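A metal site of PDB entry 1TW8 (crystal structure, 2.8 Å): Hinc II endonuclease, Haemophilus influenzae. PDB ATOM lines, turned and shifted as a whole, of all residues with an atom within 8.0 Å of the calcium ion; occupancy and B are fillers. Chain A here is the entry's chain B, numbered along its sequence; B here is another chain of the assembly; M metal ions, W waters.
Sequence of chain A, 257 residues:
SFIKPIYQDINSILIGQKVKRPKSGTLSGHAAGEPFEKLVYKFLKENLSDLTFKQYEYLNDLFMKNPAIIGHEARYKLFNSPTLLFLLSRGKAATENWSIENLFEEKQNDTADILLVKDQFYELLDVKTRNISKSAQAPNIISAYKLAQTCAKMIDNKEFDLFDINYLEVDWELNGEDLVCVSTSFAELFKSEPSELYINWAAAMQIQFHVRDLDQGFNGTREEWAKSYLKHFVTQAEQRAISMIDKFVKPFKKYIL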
ATOM      1  N   HIS A  30      25.160  -8.710  35.397  1.00  0.00           N
ATOM      2  CA  HIS A  30      25.405  -9.812  34.479  1.00  0.00           C
ATOM      3  C   HIS A  30      24.193 -10.757  34.405  1.00  0.00           C
ATOM      4  O   HIS A  30      24.088 -11.568  33.487  1.00  0.00           O
ATOM      5  CB  HIS A  30      26.659 -10.577  34.918  1.00  0.00           C
ATOM      6  CG  HIS A  30      27.817 -10.404  33.980  1.00  0.00           C
ATOM      7  ND1 HIS A  30      27.885 -11.033  32.756  1.00  0.00           N
ATOM      8  CD2 HIS A  30      28.953  -9.665  34.087  1.00  0.00           C
ATOM      9  CE1 HIS A  30      29.004 -10.679  32.141  1.00  0.00           C
ATOM     10  NE2 HIS A  30      29.668  -9.855  32.928  1.00  0.00           N
ATOM     11  N   GLU A  34      21.024  -9.629  30.105  1.00  0.00           N
ATOM     12  CA  GLU A  34      22.170 -10.303  29.527  1.00  0.00           C
ATOM     13  C   GLU A  34      21.805 -11.252  28.380  1.00  0.00           C
ATOM     14  O   GLU A  34      22.264 -11.068  27.261  1.00  0.00           O
ATOM     15  CB  GLU A  34      22.926 -11.086  30.601  1.00  0.00           C
ATOM     16  CG  GLU A  34      24.095 -11.903  30.090  1.00  0.00           C
ATOM     17  CD  GLU A  34      25.356 -11.065  29.953  1.00  0.00           C
ATOM     18  OE1 GLU A  34      25.242  -9.890  29.560  1.00  0.00           O
ATOM     19  OE2 GLU A  34      26.455 -11.611  30.219  1.00  0.00           O
ATOM     20  N   GLU A  37      21.781 -10.652  24.553  1.00  0.00           N
ATOM     21  CA  GLU A  37      22.942 -10.549  23.691  1.00  0.00           C
ATOM     22  C   GLU A  37      23.007 -11.868  22.926  1.00  0.00           C
ATOM     23  O   GLU A  37      23.515 -11.924  21.810  1.00  0.00           O
ATOM     24  CB  GLU A  37      24.233 -10.315  24.487  1.00  0.00           C
ATOM     25  CG  GLU A  37      24.959 -11.570  24.931  1.00  0.00           C
ATOM     26  CD  GLU A  37      26.332 -11.689  24.292  1.00  0.00           C
ATOM     27  OE1 GLU A  37      26.411 -11.729  23.047  1.00  0.00           O
ATOM     28  OE2 GLU A  37      27.332 -11.743  25.039  1.00  0.00           O
ATOM     29  N   ASP A 110      36.180  -9.455  27.846  1.00  0.00           N
ATOM     30  CA  ASP A 110      36.431  -9.358  26.418  1.00  0.00           C
ATOM     31  C   ASP A 110      35.796  -8.095  25.873  1.00  0.00           C
ATOM     32  O   ASP A 110      34.591  -7.878  26.041  1.00  0.00           O
ATOM     33  CB  ASP A 110      35.901 -10.583  25.657  1.00  0.00           C
ATOM     34  CG  ASP A 110      36.822 -11.796  25.791  1.00  0.00           C
ATOM     35  OD1 ASP A 110      38.036 -11.631  26.004  1.00  0.00           O
ATOM     36  OD2 ASP A 110      36.330 -12.934  25.679  1.00  0.00           O
ATOM     37  N   THR A 111      36.624  -7.278  25.248  1.00  0.00           N
ATOM     38  CA  THR A 111      36.208  -6.014  24.641  1.00  0.00           C
ATOM     39  C   THR A 111      34.835  -6.081  23.968  1.00  0.00           C
ATOM     40  O   THR A 111      33.950  -5.298  24.295  1.00  0.00           O
ATOM     41  CB  THR A 111      37.234  -5.552  23.589  1.00  0.00           C
ATOM     42  OG1 THR A 111      38.505  -5.333  24.216  1.00  0.00           O
ATOM     43  CG2 THR A 111      36.767  -4.271  22.904  1.00  0.00           C
ATOM     44  N   ALA A 112      34.661  -7.033  23.057  1.00  0.00           N
ATOM     45  CA  ALA A 112      33.392  -7.120  22.338  1.00  0.00           C
ATOM     46  C   ALA A 112      32.486  -8.305  22.616  1.00  0.00           C
ATOM     47  O   ALA A 112      32.929  -9.331  23.106  1.00  0.00           O
ATOM     48  CB  ALA A 112      33.648  -7.030  20.846  1.00  0.00           C
ATOM     49  N   ASP A 113      31.221  -8.153  22.295  1.00  0.00           N
ATOM     50  CA  ASP A 113      30.286  -9.244  22.473  1.00  0.00           C
ATOM     51  C   ASP A 113      30.289 -10.015  21.163  1.00  0.00           C
ATOM     52  O   ASP A 113      30.261 -11.240  21.162  1.00  0.00           O
ATOM     53  CB  ASP A 113      28.878  -8.721  22.757  1.00  0.00           C
ATOM     54  CG  ASP A 113      28.673  -8.334  24.221  1.00  0.00           C
ATOM     55  OD1 ASP A 113      27.714  -7.561  24.494  1.00  0.00           O
ATOM     56  OD2 ASP A 113      29.432  -8.798  25.095  1.00  0.00           O
ATOM     57  N   ILE A 114      30.337  -9.288  20.053  1.00  0.00           N
ATOM     58  CA  ILE A 114      30.312  -9.892  18.733  1.00  0.00           C
ATOM     59  C   ILE A 114      31.306  -9.195  17.810  1.00  0.00           C
ATOM     60  O   ILE A 114      31.448  -7.987  17.837  1.00  0.00           O
ATOM     61  CB  ILE A 114      28.908  -9.787  18.122  1.00  0.00           C
ATOM     62  CG1 ILE A 114      27.919 -10.506  19.040  1.00  0.00           C
ATOM     63  CG2 ILE A 114      28.890 -10.380  16.722  1.00  0.00           C
ATOM     64  CD1 ILE A 114      26.515 -10.494  18.541  1.00  0.00           C
ATOM     65  N   LEU A 125      31.243  -5.145  18.171  1.00  0.00           N
ATOM     66  CA  LEU A 125      29.902  -4.798  18.639  1.00  0.00           C
ATOM     67  C   LEU A 125      29.669  -5.171  20.113  1.00  0.00           C
ATOM     68  O   LEU A 125      29.865  -6.305  20.515  1.00  0.00           O
ATOM     69  CB  LEU A 125      28.869  -5.519  17.785  1.00  0.00           C
ATOM     70  CG  LEU A 125      27.400  -5.290  18.132  1.00  0.00           C
ATOM     71  CD1 LEU A 125      26.958  -3.896  17.721  1.00  0.00           C
ATOM     72  CD2 LEU A 125      26.568  -6.346  17.433  1.00  0.00           C
ATOM     73  N   ASP A 126      29.231  -4.203  20.906  1.00  0.00           N
ATOM     74  CA  ASP A 126      28.957  -4.461  22.315  1.00  0.00           C
ATOM     75  C   ASP A 126      27.489  -4.193  22.558  1.00  0.00           C
ATOM     76  O   ASP A 126      27.032  -3.050  22.467  1.00  0.00           O
ATOM     77  CB  ASP A 126      29.804  -3.529  23.190  1.00  0.00           C
ATOM     78  CG  ASP A 126      29.546  -3.716  24.688  1.00  0.00           C
ATOM     79  OD1 ASP A 126      30.302  -3.121  25.481  1.00  0.00           O
ATOM     80  OD2 ASP A 126      28.600  -4.442  25.079  1.00  0.00           O
ATOM     81  N   VAL A 127      26.752  -5.257  22.876  1.00  0.00           N
ATOM     82  CA  VAL A 127      25.314  -5.126  23.127  1.00  0.00           C
ATOM     83  C   VAL A 127      24.992  -4.679  24.544  1.00  0.00           C
ATOM     84  O   VAL A 127      25.637  -5.098  25.490  1.00  0.00           O
ATOM     85  CB  VAL A 127      24.574  -6.442  22.827  1.00  0.00           C
ATOM     86  CG1 VAL A 127      23.103  -6.326  23.249  1.00  0.00           C
ATOM     87  CG2 VAL A 127      24.664  -6.758  21.330  1.00  0.00           C
ATOM     88  N   LYS A 128      23.982  -3.807  24.676  1.00  0.00           N
ATOM     89  CA  LYS A 128      23.550  -3.292  25.976  1.00  0.00           C
ATOM     90  C   LYS A 128      22.064  -3.593  26.193  1.00  0.00           C
ATOM     91  O   LYS A 128      21.243  -3.329  25.322  1.00  0.00           O
ATOM     92  CB  LYS A 128      23.748  -1.788  26.024  1.00  0.00           C
ATOM     93  CG  LYS A 128      25.147  -1.316  25.683  1.00  0.00           C
ATOM     94  CD  LYS A 128      26.190  -1.750  26.708  1.00  0.00           C
ATOM     95  CE  LYS A 128      27.565  -1.289  26.273  1.00  0.00           C
ATOM     96  NZ  LYS A 128      28.620  -1.657  27.231  1.00  0.00           N
ATOM     97  N   THR A 129      21.722  -4.143  27.357  1.00  0.00           N
ATOM     98  CA  THR A 129      20.318  -4.420  27.652  1.00  0.00           C
ATOM     99  C   THR A 129      19.825  -3.425  28.688  1.00  0.00           C
ATOM    100  O   THR A 129      20.614  -2.842  29.426  1.00  0.00           O
ATOM    101  CB  THR A 129      20.101  -5.830  28.183  1.00  0.00           C
ATOM    102  OG1 THR A 129      20.724  -5.958  29.447  1.00  0.00           O
ATOM    103  CG2 THR A 129      20.651  -6.849  27.223  1.00  0.00           C
ATOM    104  N   ASN A 140      27.703   1.085  31.649  1.00  0.00           N
ATOM    105  CA  ASN A 140      29.131   1.098  31.320  1.00  0.00           C
ATOM    106  C   ASN A 140      29.252   0.723  29.839  1.00  0.00           C
ATOM    107  O   ASN A 140      28.865  -0.362  29.441  1.00  0.00           O
ATOM    108  CB  ASN A 140      29.893   0.060  32.146  1.00  0.00           C
ATOM    109  CG  ASN A 140      29.962   0.408  33.631  1.00  0.00           C
ATOM    110  OD1 ASN A 140      29.345   1.375  34.084  1.00  0.00           O
ATOM    111  ND2 ASN A 140      30.710  -0.385  34.393  1.00  0.00           N
ATOM    112  N   ILE A 141      29.780   1.645  29.054  1.00  0.00           N
ATOM    113  CA  ILE A 141      29.974   1.427  27.621  1.00  0.00           C
ATOM    114  C   ILE A 141      31.300   0.692  27.429  1.00  0.00           C
ATOM    115  O   ILE A 141      31.334  -0.427  26.940  1.00  0.00           O
ATOM    116  CB  ILE A 141      30.038   2.772  26.879  1.00  0.00           C
ATOM    117  CG1 ILE A 141      28.802   3.603  27.207  1.00  0.00           C
ATOM    118  CG2 ILE A 141      30.116   2.549  25.393  1.00  0.00           C
ATOM    119  CD1 ILE A 141      27.520   2.909  26.793  1.00  0.00           C
ATOM    120  N   TYR A 167      27.607   0.109  19.202  1.00  0.00           N
ATOM    121  CA  TYR A 167      26.732  -0.406  20.231  1.00  0.00           C
ATOM    122  C   TYR A 167      25.288  -0.624  19.820  1.00  0.00           C
ATOM    123  O   TYR A 167      24.741   0.121  19.025  1.00  0.00           O
ATOM    124  CB  TYR A 167      26.819   0.522  21.425  1.00  0.00           C
ATOM    125  CG  TYR A 167      28.234   0.558  21.936  1.00  0.00           C
ATOM    126  CD1 TYR A 167      28.667  -0.318  22.925  1.00  0.00           C
ATOM    127  CD2 TYR A 167      29.132   1.485  21.430  1.00  0.00           C
ATOM    128  CE1 TYR A 167      29.963  -0.255  23.402  1.00  0.00           C
ATOM    129  CE2 TYR A 167      30.428   1.550  21.896  1.00  0.00           C
ATOM    130  CZ  TYR A 167      30.834   0.690  22.890  1.00  0.00           C
ATOM    131  OH  TYR A 167      32.091   0.855  23.412  1.00  0.00           O
ATOM    132  N   LEU A 168      24.672  -1.672  20.379  1.00  0.00           N
ATOM    133  CA  LEU A 168      23.291  -2.011  20.082  1.00  0.00           C
ATOM    134  C   LEU A 168      22.480  -2.136  21.371  1.00  0.00           C
ATOM    135  O   LEU A 168      22.544  -3.158  22.058  1.00  0.00           O
ATOM    136  CB  LEU A 168      23.214  -3.336  19.337  1.00  0.00           C
ATOM    137  CG  LEU A 168      21.795  -3.885  19.164  1.00  0.00           C
ATOM    138  CD1 LEU A 168      21.045  -3.107  18.079  1.00  0.00           C
ATOM    139  CD2 LEU A 168      21.869  -5.357  18.784  1.00  0.00           C
ATOM    140  P    DC B   7      35.914  -3.393  29.151  1.00  0.00           P
ATOM    141  OP1  DC B   7      36.308  -3.522  27.720  1.00  0.00           O
ATOM    142  OP2  DC B   7      35.662  -2.051  29.716  1.00  0.00           O
ATOM    143  O5'  DC B   7      34.636  -4.297  29.386  1.00  0.00           O
ATOM    144  C5'  DC B   7      34.765  -5.709  29.278  1.00  0.00           C
ATOM    145  C4'  DC B   7      33.601  -6.405  29.934  1.00  0.00           C
ATOM    146  O4'  DC B   7      33.805  -6.424  31.370  1.00  0.00           O
ATOM    147  C3'  DC B   7      32.293  -5.666  29.684  1.00  0.00           C
ATOM    148  O3'  DC B   7      31.313  -6.490  29.052  1.00  0.00           O
ATOM    149  C2'  DC B   7      31.796  -5.252  31.062  1.00  0.00           C
ATOM    150  C1'  DC B   7      32.584  -6.126  32.021  1.00  0.00           C
ATOM    151  N1   DC B   7      32.889  -5.382  33.252  1.00  0.00           N
ATOM    152  C2   DC B   7      32.596  -5.960  34.481  1.00  0.00           C
ATOM    153  O2   DC B   7      32.322  -7.165  34.526  1.00  0.00           O
ATOM    154  N3   DC B   7      32.637  -5.197  35.593  1.00  0.00           N
ATOM    155  C4   DC B   7      32.974  -3.914  35.504  1.00  0.00           C
ATOM    156  N4   DC B   7      32.879  -3.153  36.586  1.00  0.00           N
ATOM    157  C5   DC B   7      33.395  -3.335  34.276  1.00  0.00           C
ATOM    158  C6   DC B   7      33.348  -4.095  33.185  1.00  0.00           C
ATOM    159  P    DG B   8      30.011  -5.810  28.407  1.00  0.00           P
ATOM    160  OP1  DG B   8      29.536  -6.643  27.278  1.00  0.00           O
ATOM    161  OP2  DG B   8      30.275  -4.356  28.185  1.00  0.00           O
ATOM    162  O5'  DG B   8      28.956  -5.929  29.595  1.00  0.00           O
ATOM    163  C5'  DG B   8      28.836  -7.176  30.289  1.00  0.00           C
ATOM    164  C4'  DG B   8      27.679  -7.115  31.253  1.00  0.00           C
ATOM    165  O4'  DG B   8      28.165  -6.899  32.602  1.00  0.00           O
ATOM    166  C3'  DG B   8      26.785  -5.935  30.915  1.00  0.00           C
ATOM    167  O3'  DG B   8      25.412  -6.311  30.794  1.00  0.00           O
ATOM    168  C2'  DG B   8      26.952  -4.986  32.083  1.00  0.00           C
ATOM    169  C1'  DG B   8      27.408  -5.879  33.223  1.00  0.00           C
ATOM    170  N9   DG B   8      28.281  -5.130  34.114  1.00  0.00           N
ATOM    171  C8   DG B   8      29.371  -4.381  33.750  1.00  0.00           C
ATOM    172  N7   DG B   8      29.839  -3.648  34.720  1.00  0.00           N
ATOM    173  C5   DG B   8      29.033  -3.972  35.806  1.00  0.00           C
ATOM    174  C6   DG B   8      29.061  -3.488  37.139  1.00  0.00           C
ATOM    175  O6   DG B   8      29.760  -2.589  37.635  1.00  0.00           O
ATOM    176  N1   DG B   8      28.118  -4.136  37.929  1.00  0.00           N
ATOM    177  C2   DG B   8      27.251  -5.101  37.499  1.00  0.00           C
ATOM    178  N2   DG B   8      26.424  -5.607  38.438  1.00  0.00           N
ATOM    179  N3   DG B   8      27.186  -5.543  36.249  1.00  0.00           N
ATOM    180  C4   DG B   8      28.111  -4.937  35.459  1.00  0.00           C
ATOM    181  P    DA B   9      24.389  -5.292  30.118  1.00  0.00           P
ATOM    182  OP1  DA B   9      23.326  -6.092  29.482  1.00  0.00           O
ATOM    183  OP2  DA B   9      25.170  -4.320  29.294  1.00  0.00           O
ATOM    184  O5'  DA B   9      23.794  -4.531  31.376  1.00  0.00           O
ATOM    185  C5'  DA B   9      23.252  -5.292  32.436  1.00  0.00           C
ATOM    186  C4'  DA B   9      22.860  -4.383  33.575  1.00  0.00           C
ATOM    187  O4'  DA B   9      24.040  -3.866  34.245  1.00  0.00           O
ATOM    188  C3'  DA B   9      22.066  -3.173  33.131  1.00  0.00           C
ATOM    189  O3'  DA B   9      21.014  -2.975  34.066  1.00  0.00           O
ATOM    190  C2'  DA B   9      23.071  -2.034  33.273  1.00  0.00           C
ATOM    191  C1'  DA B   9      23.823  -2.509  34.494  1.00  0.00           C
ATOM    192  N9   DA B   9      25.100  -1.830  34.730  1.00  0.00           N
ATOM    193  C8   DA B   9      25.911  -1.256  33.788  1.00  0.00           C
ATOM    194  N7   DA B   9      26.911  -0.573  34.303  1.00  0.00           N
ATOM    195  C5   DA B   9      26.753  -0.722  35.666  1.00  0.00           C
ATOM    196  C6   DA B   9      27.480  -0.212  36.757  1.00  0.00           C
ATOM    197  N6   DA B   9      28.475   0.667  36.620  1.00  0.00           N
ATOM    198  N1   DA B   9      27.125  -0.621  38.007  1.00  0.00           N
ATOM    199  C2   DA B   9      26.078  -1.448  38.136  1.00  0.00           C
ATOM    200  N3   DA B   9      25.275  -1.959  37.168  1.00  0.00           N
ATOM    201  C4   DA B   9      25.681  -1.553  35.939  1.00  0.00           C
HETATM  202 CA    CA M   1      27.653  -6.100  26.323  1.00  0.00          CA
HETATM  203  O   HOH W   1      26.388  -7.662  27.004  1.00  0.00           O
HETATM  204  O   HOH W   2      27.585  -4.220  28.058  1.00  0.00           O
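OP2 of DG 8 of chain B is in salt-bridge range of NZ of Lys 128 (3.3 Å). The side-chain amide nitrogen (ND2) of Asn 140 sits at hydrogen-bond distance from N7 of DG 8 of chain B (3.4 Å). NE2 of His 30 sits close to O4' of DG 8 of chain B (3.3 Å). The side-chain carboxylate (OD1) of Asp 126 is in salt-bridge range of the side-chain amino group (NZ) of Lys 128 (2.8 Å). The backbone carbonyl oxygen (O) of Asp 126 sits at hydrogen-bond distance from the backbone NH (N) of Leu 168, 3.4 Å away. N of Asp 113 lies within hydrogen-bond range of O of Leu 125 (2.9 Å).
Of the 20 residues printed, 4 come within 4 Å of the calcium ion. The nearest printed residue that does not touch the calcium ion is DA 9 of chain B (4.3 Å).
The calcium ion is bound by water W1, at 2.1 Å. OP1 of DG 8 of chain B binds the calcium ion, 2.2 Å away. The calcium ion is bound by OD2 of Asp 126 (2.3 Å). OD1 of Asp 113 binds the calcium ion, at 2.3 Å. O of Val 127 binds the calcium ion, at 2.4 Å. Water W2 is bound to the calcium ion.
Water W2 lies within hydrogen-bond range of O5' of DG 8 of chain B (2.7 Å), OP2 of DA 9 of chain B (2.7 Å) and NZ of Lys 128 (2.9 Å).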
